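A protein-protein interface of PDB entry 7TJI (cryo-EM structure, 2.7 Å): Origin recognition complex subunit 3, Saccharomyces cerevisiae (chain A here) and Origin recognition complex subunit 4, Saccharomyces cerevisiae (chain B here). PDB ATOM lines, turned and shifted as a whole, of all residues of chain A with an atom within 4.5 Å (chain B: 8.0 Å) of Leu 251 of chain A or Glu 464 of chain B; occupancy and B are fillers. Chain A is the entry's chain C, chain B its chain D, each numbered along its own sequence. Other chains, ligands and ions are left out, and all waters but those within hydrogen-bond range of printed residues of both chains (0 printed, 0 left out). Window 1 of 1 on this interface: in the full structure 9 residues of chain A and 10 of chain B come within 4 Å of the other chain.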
ATOM      1  N   PHE A 213       5.633 -40.368   5.881  1.00  0.00           N
ATOM      2  CA  PHE A 213       4.663 -39.327   5.564  1.00  0.00           C
ATOM      3  C   PHE A 213       5.248 -38.218   4.705  1.00  0.00           C
ATOM      4  O   PHE A 213       4.492 -37.534   4.009  1.00  0.00           O
ATOM      5  CB  PHE A 213       4.073 -38.754   6.851  1.00  0.00           C
ATOM      6  CG  PHE A 213       3.041 -39.641   7.469  1.00  0.00           C
ATOM      7  CD1 PHE A 213       1.741 -39.648   6.988  1.00  0.00           C
ATOM      8  CD2 PHE A 213       3.376 -40.499   8.500  1.00  0.00           C
ATOM      9  CE1 PHE A 213       0.787 -40.482   7.543  1.00  0.00           C
ATOM     10  CE2 PHE A 213       2.426 -41.338   9.058  1.00  0.00           C
ATOM     11  CZ  PHE A 213       1.131 -41.326   8.581  1.00  0.00           C
ATOM     12  N   ASP A 217       3.322 -37.347   1.369  1.00  0.00           N
ATOM     13  CA  ASP A 217       2.981 -35.954   1.108  1.00  0.00           C
ATOM     14  C   ASP A 217       3.502 -35.497  -0.246  1.00  0.00           C
ATOM     15  O   ASP A 217       2.773 -34.858  -1.017  1.00  0.00           O
ATOM     16  CB  ASP A 217       3.547 -35.076   2.224  1.00  0.00           C
ATOM     17  CG  ASP A 217       2.721 -33.841   2.469  1.00  0.00           C
ATOM     18  OD1 ASP A 217       2.665 -32.972   1.577  1.00  0.00           O
ATOM     19  OD2 ASP A 217       2.130 -33.734   3.560  1.00  0.00           O
ATOM     20  N   ILE A 247      -2.555 -38.583  11.735  1.00  0.00           N
ATOM     21  CA  ILE A 247      -2.050 -38.411  10.378  1.00  0.00           C
ATOM     22  C   ILE A 247      -2.188 -36.971   9.891  1.00  0.00           C
ATOM     23  O   ILE A 247      -1.454 -36.567   8.977  1.00  0.00           O
ATOM     24  CB  ILE A 247      -2.731 -39.407   9.413  1.00  0.00           C
ATOM     25  CG1 ILE A 247      -3.937 -38.796   8.693  1.00  0.00           C
ATOM     26  CG2 ILE A 247      -3.148 -40.668  10.155  1.00  0.00           C
ATOM     27  CD1 ILE A 247      -3.754 -38.646   7.200  1.00  0.00           C
ATOM     28  N   GLU A 248      -3.093 -36.179  10.474  1.00  0.00           N
ATOM     29  CA  GLU A 248      -3.142 -34.771  10.112  1.00  0.00           C
ATOM     30  C   GLU A 248      -2.028 -33.975  10.776  1.00  0.00           C
ATOM     31  O   GLU A 248      -1.669 -32.905  10.280  1.00  0.00           O
ATOM     32  CB  GLU A 248      -4.516 -34.170  10.440  1.00  0.00           C
ATOM     33  CG  GLU A 248      -4.625 -33.422  11.754  1.00  0.00           C
ATOM     34  CD  GLU A 248      -6.066 -33.216  12.179  1.00  0.00           C
ATOM     35  OE1 GLU A 248      -6.863 -34.169  12.066  1.00  0.00           O
ATOM     36  OE2 GLU A 248      -6.401 -32.100  12.630  1.00  0.00           O
ATOM     37  N   LYS A 249      -1.457 -34.488  11.867  1.00  0.00           N
ATOM     38  CA  LYS A 249      -0.271 -33.877  12.446  1.00  0.00           C
ATOM     39  C   LYS A 249       1.001 -34.219  11.677  1.00  0.00           C
ATOM     40  O   LYS A 249       2.043 -33.609  11.931  1.00  0.00           O
ATOM     41  CB  LYS A 249      -0.125 -34.305  13.908  1.00  0.00           C
ATOM     42  CG  LYS A 249       0.487 -33.253  14.811  1.00  0.00           C
ATOM     43  CD  LYS A 249       0.566 -33.738  16.247  1.00  0.00           C
ATOM     44  CE  LYS A 249      -0.672 -33.346  17.038  1.00  0.00           C
ATOM     45  NZ  LYS A 249      -1.298 -32.098  16.518  1.00  0.00           N
ATOM     46  N   ASN A 250       0.938 -35.167  10.744  1.00  0.00           N
ATOM     47  CA  ASN A 250       2.106 -35.641  10.017  1.00  0.00           C
ATOM     48  C   ASN A 250       2.187 -35.114   8.593  1.00  0.00           C
ATOM     49  O   ASN A 250       3.249 -35.217   7.974  1.00  0.00           O
ATOM     50  CB  ASN A 250       2.118 -37.172   9.990  1.00  0.00           C
ATOM     51  CG  ASN A 250       2.789 -37.765  11.204  1.00  0.00           C
ATOM     52  OD1 ASN A 250       3.486 -37.071  11.941  1.00  0.00           O
ATOM     53  ND2 ASN A 250       2.576 -39.053  11.425  1.00  0.00           N
ATOM     54  N   LEU A 251       1.105 -34.566   8.058  1.00  0.00           N
ATOM     55  CA  LEU A 251       1.113 -33.963   6.736  1.00  0.00           C
ATOM     56  C   LEU A 251       1.298 -32.455   6.847  1.00  0.00           C
ATOM     57  O   LEU A 251       1.180 -31.862   7.921  1.00  0.00           O
ATOM     58  CB  LEU A 251      -0.181 -34.281   5.981  1.00  0.00           C
ATOM     59  CG  LEU A 251      -0.514 -35.741   5.680  1.00  0.00           C
ATOM     60  CD1 LEU A 251      -1.727 -35.821   4.772  1.00  0.00           C
ATOM     61  CD2 LEU A 251       0.674 -36.454   5.056  1.00  0.00           C
ATOM     62  N   ARG A 252       1.596 -31.838   5.710  1.00  0.00           N
ATOM     63  CA  ARG A 252       1.674 -30.389   5.645  1.00  0.00           C
ATOM     64  C   ARG A 252       0.278 -29.777   5.714  1.00  0.00           C
ATOM     65  O   ARG A 252      -0.725 -30.407   5.374  1.00  0.00           O
ATOM     66  CB  ARG A 252       2.374 -29.940   4.364  1.00  0.00           C
ATOM     67  CG  ARG A 252       3.888 -29.949   4.440  1.00  0.00           C
ATOM     68  CD  ARG A 252       4.504 -29.428   3.151  1.00  0.00           C
ATOM     69  NE  ARG A 252       4.356 -30.367   2.047  1.00  0.00           N
ATOM     70  CZ  ARG A 252       5.315 -31.175   1.618  1.00  0.00           C
ATOM     71  NH1 ARG A 252       6.513 -31.184   2.180  1.00  0.00           N
ATOM     72  NH2 ARG A 252       5.067 -31.996   0.600  1.00  0.00           N
ATOM     73  N   GLN A 253       0.232 -28.521   6.168  1.00  0.00           N
ATOM     74  CA  GLN A 253      -1.023 -27.784   6.247  1.00  0.00           C
ATOM     75  C   GLN A 253      -1.622 -27.529   4.869  1.00  0.00           C
ATOM     76  O   GLN A 253      -2.850 -27.531   4.717  1.00  0.00           O
ATOM     77  CB  GLN A 253      -0.796 -26.466   6.985  1.00  0.00           C
ATOM     78  CG  GLN A 253      -2.034 -25.892   7.620  1.00  0.00           C
ATOM     79  CD  GLN A 253      -2.708 -26.865   8.547  1.00  0.00           C
ATOM     80  OE1 GLN A 253      -3.776 -27.392   8.242  1.00  0.00           O
ATOM     81  NE2 GLN A 253      -2.087 -27.115   9.690  1.00  0.00           N
ATOM     82  N   THR A 255      -1.256 -29.652   2.415  1.00  0.00           N
ATOM     83  CA  THR A 255      -1.805 -30.959   2.063  1.00  0.00           C
ATOM     84  C   THR A 255      -3.150 -31.204   2.746  1.00  0.00           C
ATOM     85  O   THR A 255      -4.053 -31.798   2.145  1.00  0.00           O
ATOM     86  CB  THR A 255      -0.809 -32.060   2.425  1.00  0.00           C
ATOM     87  OG1 THR A 255       0.514 -31.635   2.085  1.00  0.00           O
ATOM     88  CG2 THR A 255      -1.130 -33.345   1.671  1.00  0.00           C
ATOM     89  N   ILE A 256      -3.293 -30.759   3.999  1.00  0.00           N
ATOM     90  CA  ILE A 256      -4.569 -30.869   4.702  1.00  0.00           C
ATOM     91  C   ILE A 256      -5.629 -30.016   4.016  1.00  0.00           C
ATOM     92  O   ILE A 256      -6.771 -30.456   3.830  1.00  0.00           O
ATOM     93  CB  ILE A 256      -4.397 -30.488   6.187  1.00  0.00           C
ATOM     94  CG1 ILE A 256      -3.454 -31.463   6.893  1.00  0.00           C
ATOM     95  CG2 ILE A 256      -5.735 -30.446   6.914  1.00  0.00           C
ATOM     96  CD1 ILE A 256      -3.941 -32.887   6.904  1.00  0.00           C
ATOM     97  N   LEU A 259      -6.688 -31.910   0.874  1.00  0.00           N
ATOM     98  CA  LEU A 259      -7.519 -33.090   1.083  1.00  0.00           C
ATOM     99  C   LEU A 259      -8.907 -32.755   1.616  1.00  0.00           C
ATOM    100  O   LEU A 259      -9.823 -33.571   1.477  1.00  0.00           O
ATOM    101  CB  LEU A 259      -6.816 -34.061   2.034  1.00  0.00           C
ATOM    102  CG  LEU A 259      -5.539 -34.720   1.503  1.00  0.00           C
ATOM    103  CD1 LEU A 259      -4.862 -35.558   2.571  1.00  0.00           C
ATOM    104  CD2 LEU A 259      -5.834 -35.549   0.267  1.00  0.00           C
ATOM    105  N   GLU B 390       4.723 -14.318  11.027  1.00  0.00           N
ATOM    106  CA  GLU B 390       5.926 -14.943  10.480  1.00  0.00           C
ATOM    107  C   GLU B 390       7.191 -14.329  11.066  1.00  0.00           C
ATOM    108  O   GLU B 390       8.116 -15.053  11.462  1.00  0.00           O
ATOM    109  CB  GLU B 390       5.932 -14.813   8.958  1.00  0.00           C
ATOM    110  CG  GLU B 390       5.269 -15.957   8.234  1.00  0.00           C
ATOM    111  CD  GLU B 390       4.625 -15.533   6.932  1.00  0.00           C
ATOM    112  OE1 GLU B 390       4.857 -14.390   6.489  1.00  0.00           O
ATOM    113  OE2 GLU B 390       3.874 -16.347   6.357  1.00  0.00           O
ATOM    114  N   ILE B 393       7.506 -15.385  14.821  1.00  0.00           N
ATOM    115  CA  ILE B 393       7.961 -16.768  14.956  1.00  0.00           C
ATOM    116  C   ILE B 393       9.441 -16.888  14.600  1.00  0.00           C
ATOM    117  O   ILE B 393      10.203 -17.586  15.285  1.00  0.00           O
ATOM    118  CB  ILE B 393       7.076 -17.700  14.101  1.00  0.00           C
ATOM    119  CG1 ILE B 393       5.672 -17.796  14.695  1.00  0.00           C
ATOM    120  CG2 ILE B 393       7.648 -19.099  14.013  1.00  0.00           C
ATOM    121  CD1 ILE B 393       5.649 -18.187  16.147  1.00  0.00           C
ATOM    122  N   PHE B 411      10.056 -26.756  17.078  1.00  0.00           N
ATOM    123  CA  PHE B 411       8.815 -25.992  17.043  1.00  0.00           C
ATOM    124  C   PHE B 411       8.292 -25.689  18.444  1.00  0.00           C
ATOM    125  O   PHE B 411       7.713 -24.619  18.666  1.00  0.00           O
ATOM    126  CB  PHE B 411       7.781 -26.768  16.224  1.00  0.00           C
ATOM    127  CG  PHE B 411       6.443 -26.105  16.128  1.00  0.00           C
ATOM    128  CD1 PHE B 411       6.226 -25.100  15.206  1.00  0.00           C
ATOM    129  CD2 PHE B 411       5.389 -26.511  16.938  1.00  0.00           C
ATOM    130  CE1 PHE B 411       4.996 -24.498  15.104  1.00  0.00           C
ATOM    131  CE2 PHE B 411       4.158 -25.905  16.845  1.00  0.00           C
ATOM    132  CZ  PHE B 411       3.959 -24.899  15.927  1.00  0.00           C
ATOM    133  N   LYS B 457      -1.619 -25.041  16.434  1.00  0.00           N
ATOM    134  CA  LYS B 457      -2.248 -25.556  15.223  1.00  0.00           C
ATOM    135  C   LYS B 457      -2.128 -24.572  14.064  1.00  0.00           C
ATOM    136  O   LYS B 457      -1.892 -24.975  12.920  1.00  0.00           O
ATOM    137  CB  LYS B 457      -3.713 -25.875  15.531  1.00  0.00           C
ATOM    138  CG  LYS B 457      -4.647 -25.952  14.336  1.00  0.00           C
ATOM    139  CD  LYS B 457      -5.922 -25.143  14.561  1.00  0.00           C
ATOM    140  CE  LYS B 457      -6.538 -25.402  15.930  1.00  0.00           C
ATOM    141  NZ  LYS B 457      -7.553 -24.375  16.287  1.00  0.00           N
ATOM    142  N   ASP B 458      -2.244 -23.276  14.345  1.00  0.00           N
ATOM    143  CA  ASP B 458      -2.122 -22.266  13.307  1.00  0.00           C
ATOM    144  C   ASP B 458      -0.689 -21.805  13.086  1.00  0.00           C
ATOM    145  O   ASP B 458      -0.372 -21.302  12.003  1.00  0.00           O
ATOM    146  CB  ASP B 458      -3.003 -21.064  13.645  1.00  0.00           C
ATOM    147  CG  ASP B 458      -4.347 -21.135  12.971  1.00  0.00           C
ATOM    148  OD1 ASP B 458      -4.927 -22.239  12.920  1.00  0.00           O
ATOM    149  OD2 ASP B 458      -4.821 -20.091  12.480  1.00  0.00           O
ATOM    150  N   VAL B 459       0.182 -21.967  14.083  1.00  0.00           N
ATOM    151  CA  VAL B 459       1.585 -21.610  13.933  1.00  0.00           C
ATOM    152  C   VAL B 459       2.324 -22.685  13.131  1.00  0.00           C
ATOM    153  O   VAL B 459       3.387 -22.411  12.554  1.00  0.00           O
ATOM    154  CB  VAL B 459       2.128 -21.327  15.357  1.00  0.00           C
ATOM    155  CG1 VAL B 459       3.636 -21.214  15.443  1.00  0.00           C
ATOM    156  CG2 VAL B 459       1.526 -20.034  15.878  1.00  0.00           C
ATOM    157  N   LYS B 460       1.739 -23.890  13.041  1.00  0.00           N
ATOM    158  CA  LYS B 460       2.257 -24.963  12.187  1.00  0.00           C
ATOM    159  C   LYS B 460       2.412 -24.533  10.728  1.00  0.00           C
ATOM    160  O   LYS B 460       3.424 -24.844  10.083  1.00  0.00           O
ATOM    161  CB  LYS B 460       1.319 -26.169  12.286  1.00  0.00           C
ATOM    162  CG  LYS B 460       1.888 -27.476  11.770  1.00  0.00           C
ATOM    163  CD  LYS B 460       1.045 -28.083  10.678  1.00  0.00           C
ATOM    164  CE  LYS B 460       1.479 -29.510  10.389  1.00  0.00           C
ATOM    165  NZ  LYS B 460       1.148 -30.450  11.490  1.00  0.00           N
ATOM    166  N   ASN B 461       1.434 -23.785  10.207  1.00  0.00           N
ATOM    167  CA  ASN B 461       1.471 -23.316   8.824  1.00  0.00           C
ATOM    168  C   ASN B 461       2.584 -22.299   8.600  1.00  0.00           C
ATOM    169  O   ASN B 461       3.299 -22.364   7.593  1.00  0.00           O
ATOM    170  CB  ASN B 461       0.114 -22.718   8.455  1.00  0.00           C
ATOM    171  CG  ASN B 461      -0.013 -22.413   6.982  1.00  0.00           C
ATOM    172  OD1 ASN B 461      -0.109 -23.317   6.155  1.00  0.00           O
ATOM    173  ND2 ASN B 461      -0.034 -21.132   6.645  1.00  0.00           N
ATOM    174  N   VAL B 462       2.735 -21.352   9.530  1.00  0.00           N
ATOM    175  CA  VAL B 462       3.784 -20.339   9.443  1.00  0.00           C
ATOM    176  C   VAL B 462       5.161 -20.987   9.558  1.00  0.00           C
ATOM    177  O   VAL B 462       6.106 -20.606   8.853  1.00  0.00           O
ATOM    178  CB  VAL B 462       3.534 -19.261  10.520  1.00  0.00           C
ATOM    179  CG1 VAL B 462       4.802 -18.524  10.921  1.00  0.00           C
ATOM    180  CG2 VAL B 462       2.488 -18.277  10.031  1.00  0.00           C
ATOM    181  N   TRP B 463       5.273 -22.016  10.402  1.00  0.00           N
ATOM    182  CA  TRP B 463       6.506 -22.786  10.526  1.00  0.00           C
ATOM    183  C   TRP B 463       6.863 -23.490   9.221  1.00  0.00           C
ATOM    184  O   TRP B 463       8.030 -23.483   8.799  1.00  0.00           O
ATOM    185  CB  TRP B 463       6.351 -23.804  11.650  1.00  0.00           C
ATOM    186  CG  TRP B 463       7.598 -24.516  12.014  1.00  0.00           C
ATOM    187  CD1 TRP B 463       8.010 -25.730  11.562  1.00  0.00           C
ATOM    188  CD2 TRP B 463       8.597 -24.065  12.926  1.00  0.00           C
ATOM    189  NE1 TRP B 463       9.209 -26.064  12.133  1.00  0.00           N
ATOM    190  CE2 TRP B 463       9.591 -25.056  12.977  1.00  0.00           C
ATOM    191  CE3 TRP B 463       8.748 -22.919  13.706  1.00  0.00           C
ATOM    192  CZ2 TRP B 463      10.718 -24.935  13.776  1.00  0.00           C
ATOM    193  CZ3 TRP B 463       9.865 -22.801  14.494  1.00  0.00           C
ATOM    194  CH2 TRP B 463      10.832 -23.803  14.529  1.00  0.00           C
ATOM    195  N   GLU B 464       5.864 -24.086   8.565  1.00  0.00           N
ATOM    196  CA  GLU B 464       6.099 -24.749   7.288  1.00  0.00           C
ATOM    197  C   GLU B 464       6.499 -23.755   6.202  1.00  0.00           C
ATOM    198  O   GLU B 464       7.367 -24.058   5.375  1.00  0.00           O
ATOM    199  CB  GLU B 464       4.862 -25.542   6.878  1.00  0.00           C
ATOM    200  CG  GLU B 464       4.885 -26.959   7.404  1.00  0.00           C
ATOM    201  CD  GLU B 464       3.509 -27.561   7.569  1.00  0.00           C
ATOM    202  OE1 GLU B 464       2.505 -26.843   7.386  1.00  0.00           O
ATOM    203  OE2 GLU B 464       3.439 -28.760   7.894  1.00  0.00           O
ATOM    204  N   ASN B 465       5.888 -22.565   6.198  1.00  0.00           N
ATOM    205  CA  ASN B 465       6.277 -21.527   5.246  1.00  0.00           C
ATOM    206  C   ASN B 465       7.697 -21.033   5.497  1.00  0.00           C
ATOM    207  O   ASN B 465       8.425 -20.720   4.548  1.00  0.00           O
ATOM    208  CB  ASN B 465       5.302 -20.352   5.298  1.00  0.00           C
ATOM    209  CG  ASN B 465       3.881 -20.756   4.997  1.00  0.00           C
ATOM    210  OD1 ASN B 465       3.635 -21.725   4.283  1.00  0.00           O
ATOM    211  ND2 ASN B 465       2.930 -20.012   5.544  1.00  0.00           N
ATOM    212  N   LEU B 466       8.103 -20.937   6.765  1.00  0.00           N
ATOM    213  CA  LEU B 466       9.458 -20.492   7.080  1.00  0.00           C
ATOM    214  C   LEU B 466      10.492 -21.535   6.678  1.00  0.00           C
ATOM    215  O   LEU B 466      11.604 -21.183   6.269  1.00  0.00           O
ATOM    216  CB  LEU B 466       9.579 -20.162   8.568  1.00  0.00           C
ATOM    217  CG  LEU B 466       9.008 -18.817   9.016  1.00  0.00           C
ATOM    218  CD1 LEU B 466       9.009 -18.714  10.526  1.00  0.00           C
ATOM    219  CD2 LEU B 466       9.780 -17.666   8.402  1.00  0.00           C
ATOM    220  N   VAL B 467      10.155 -22.821   6.810  1.00  0.00           N
ATOM    221  CA  VAL B 467      11.034 -23.870   6.296  1.00  0.00           C
ATOM    222  C   VAL B 467      11.089 -23.814   4.770  1.00  0.00           C
ATOM    223  O   VAL B 467      12.157 -23.973   4.166  1.00  0.00           O
ATOM    224  CB  VAL B 467      10.575 -25.248   6.815  1.00  0.00           C
ATOM    225  CG1 VAL B 467      11.362 -26.382   6.169  1.00  0.00           C
ATOM    226  CG2 VAL B 467      10.724 -25.317   8.321  1.00  0.00           C
ATOM    227  N   GLN B 468       9.949 -23.536   4.134  1.00  0.00           N
ATOM    228  CA  GLN B 468       9.857 -23.495   2.678  1.00  0.00           C
ATOM    229  C   GLN B 468      10.665 -22.342   2.084  1.00  0.00           C
ATOM    230  O   GLN B 468      11.290 -22.496   1.029  1.00  0.00           O
ATOM    231  CB  GLN B 468       8.382 -23.404   2.275  1.00  0.00           C
ATOM    232  CG  GLN B 468       8.110 -23.161   0.805  1.00  0.00           C
ATOM    233  CD  GLN B 468       7.079 -24.113   0.238  1.00  0.00           C
ATOM    234  OE1 GLN B 468       7.306 -25.321   0.169  1.00  0.00           O
ATOM    235  NE2 GLN B 468       5.933 -23.574  -0.169  1.00  0.00           N
ATOM    236  N   LEU B 469      10.696 -21.192   2.758  1.00  0.00           N
ATOM    237  CA  LEU B 469      11.427 -20.029   2.272  1.00  0.00           C
ATOM    238  C   LEU B 469      12.891 -20.016   2.701  1.00  0.00           C
ATOM    239  O   LEU B 469      13.529 -18.959   2.617  1.00  0.00           O
ATOM    240  CB  LEU B 469      10.743 -18.742   2.732  1.00  0.00           C
ATOM    241  CG  LEU B 469       9.461 -18.372   1.982  1.00  0.00           C
ATOM    242  CD1 LEU B 469       8.692 -17.306   2.727  1.00  0.00           C
ATOM    243  CD2 LEU B 469       9.787 -17.918   0.574  1.00  0.00           C
ATOM    244  N   ASP B 470      13.417 -21.159   3.168  1.00  0.00           N
ATOM    245  CA  ASP B 470      14.834 -21.360   3.502  1.00  0.00           C
ATOM    246  C   ASP B 470      15.313 -20.409   4.600  1.00  0.00           C
ATOM    247  O   ASP B 470      16.442 -19.920   4.580  1.00  0.00           O
ATOM    248  CB  ASP B 470      15.723 -21.259   2.257  1.00  0.00           C
ATOM    249  CG  ASP B 470      17.023 -22.024   2.400  1.00  0.00           C
ATOM    250  OD1 ASP B 470      17.065 -22.989   3.188  1.00  0.00           O
ATOM    251  OD2 ASP B 470      18.007 -21.656   1.724  1.00  0.00           O
ATOM    252  N   PHE B 472      14.713 -21.575   7.947  1.00  0.00           N
ATOM    253  CA  PHE B 472      15.177 -22.674   8.775  1.00  0.00           C
ATOM    254  C   PHE B 472      15.686 -23.778   7.866  1.00  0.00           C
ATOM    255  O   PHE B 472      15.249 -23.905   6.721  1.00  0.00           O
ATOM    256  CB  PHE B 472      14.064 -23.243   9.662  1.00  0.00           C
ATOM    257  CG  PHE B 472      13.325 -22.225  10.480  1.00  0.00           C
ATOM    258  CD1 PHE B 472      13.969 -21.122  11.018  1.00  0.00           C
ATOM    259  CD2 PHE B 472      11.971 -22.397  10.734  1.00  0.00           C
ATOM    260  CE1 PHE B 472      13.274 -20.204  11.770  1.00  0.00           C
ATOM    261  CE2 PHE B 472      11.272 -21.480  11.491  1.00  0.00           C
ATOM    262  CZ  PHE B 472      11.922 -20.382  12.008  1.00  0.00           C
ATOM    263  N   PHE B 502       6.790 -33.558  13.769  1.00  0.00           N
ATOM    264  CA  PHE B 502       7.371 -32.308  13.280  1.00  0.00           C
ATOM    265  C   PHE B 502       7.783 -31.367  14.408  1.00  0.00           C
ATOM    266  O   PHE B 502       8.682 -30.543  14.220  1.00  0.00           O
ATOM    267  CB  PHE B 502       6.379 -31.605  12.342  1.00  0.00           C
ATOM    268  CG  PHE B 502       5.403 -30.712  13.055  1.00  0.00           C
ATOM    269  CD1 PHE B 502       4.338 -31.260  13.754  1.00  0.00           C
ATOM    270  CD2 PHE B 502       5.556 -29.328  13.045  1.00  0.00           C
ATOM    271  CE1 PHE B 502       3.445 -30.453  14.424  1.00  0.00           C
ATOM    272  CE2 PHE B 502       4.675 -28.523  13.724  1.00  0.00           C
ATOM    273  CZ  PHE B 502       3.617 -29.084  14.412  1.00  0.00           C
ATOM    274  N   ARG B 505      11.572 -32.018  15.455  1.00  0.00           N
ATOM    275  CA  ARG B 505      12.658 -31.967  14.482  1.00  0.00           C
ATOM    276  C   ARG B 505      13.615 -30.823  14.796  1.00  0.00           C
ATOM    277  O   ARG B 505      13.188 -29.695  15.054  1.00  0.00           O
ATOM    278  CB  ARG B 505      12.104 -31.795  13.070  1.00  0.00           C
ATOM    279  CG  ARG B 505      11.317 -32.967  12.550  1.00  0.00           C
ATOM    280  CD  ARG B 505      10.664 -32.627  11.227  1.00  0.00           C
ATOM    281  NE  ARG B 505       9.765 -33.682  10.780  1.00  0.00           N
ATOM    282  CZ  ARG B 505       8.691 -33.481  10.031  1.00  0.00           C
ATOM    283  NH1 ARG B 505       8.357 -32.272   9.609  1.00  0.00           N
ATOM    284  NH2 ARG B 505       7.933 -34.519   9.696  1.00  0.00           N
ATOM    285  N   TYR B 507      16.203 -27.938  14.010  1.00  0.00           N
ATOM    286  CA  TYR B 507      16.434 -26.991  12.932  1.00  0.00           C
ATOM    287  C   TYR B 507      17.530 -26.018  13.339  1.00  0.00           C
ATOM    288  O   TYR B 507      17.829 -25.849  14.519  1.00  0.00           O
ATOM    289  CB  TYR B 507      15.157 -26.222  12.567  1.00  0.00           C
ATOM    290  CG  TYR B 507      14.179 -27.008  11.727  1.00  0.00           C
ATOM    291  CD1 TYR B 507      14.242 -26.979  10.342  1.00  0.00           C
ATOM    292  CD2 TYR B 507      13.188 -27.775  12.319  1.00  0.00           C
ATOM    293  CE1 TYR B 507      13.354 -27.699   9.569  1.00  0.00           C
ATOM    294  CE2 TYR B 507      12.293 -28.493  11.558  1.00  0.00           C
ATOM    295  CZ  TYR B 507      12.379 -28.453  10.185  1.00  0.00           C
ATOM    296  OH  TYR B 507      11.486 -29.169   9.427  1.00  0.00           O
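The side-chain carboxylate (OE1) of Glu 464 of chain B is in hydrogen-bond range of the backbone NH (N) of Gln 253 of chain A (3.1 Å).
NZ of Lys 460 of chain B sits at hydrogen-bond distance from O of Lys 249 of chain A, at 3.3 Å.
Among the printed residues, merely in contact across the chains: Glu 248 of chain A with Lys 460 of chain B (3.9 Å), Lys 249 of chain A with Phe 502 of chain B (3.8 Å), Leu 251 of chain A with Lys 460 of chain B (3.4 Å), Leu 251 of chain A with Glu 464 of chain B (3.8 Å), Arg 252 of chain A with Glu 464 of chain B (3.3 Å), Gln 253 of chain A with Lys 457 of chain B (3.9 Å), Gln 253 of chain A with Lys 460 of chain B (3.4 Å) and Gln 253 of chain A with Asn 461 of chain B (3.3 Å).
Leu 251 of chain A touches two residues of chain B.
Printed residues of chain B within 4 Å of Gln 253 of chain A: Lys 457 (3.9 Å), Lys 460 (3.4 Å), Asn 461 (3.3 Å) and Glu 464 (3.1 Å).
Printed residues of chain A within 4 Å of Asn 461 of chain B: Gln 253 (3.3 Å).
Glu 464 of chain B touches just these residues of chain A: Leu 251, Arg 252 and Gln 253.
Asn 465 of chain B touches none of the printed residues of chain A.
Leu 466 of chain B touches none of the printed residues of chain A.
The nearest printed residue of chain A that does not touch Glu 464 of chain B is Asn 250 of chain A (6.5 Å).
The backbone carbonyl oxygen (O) of Asn 461 of chain B sits close to the side-chain amide nitrogen (ND2) of Asn 465 of chain B (3.1 Å).
The side-chain carboxylate of Asp 217 of chain A is in salt-bridge range of the guanidinium group of Arg 252 of chain A (2.8 Å).
Hydrophobic or aromatic side chains of chain B within 4 Å of the printed part of chain A: Phe 502.
Printed residues of chain A that touch a printed residue of chain B: Glu 248, Lys 249, Leu 251, Arg 252 and Gln 253.
Among the printed residues, no Asp or Glu carboxylate lies within 4 Å of a Lys or Arg side-chain nitrogen of the other chain.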
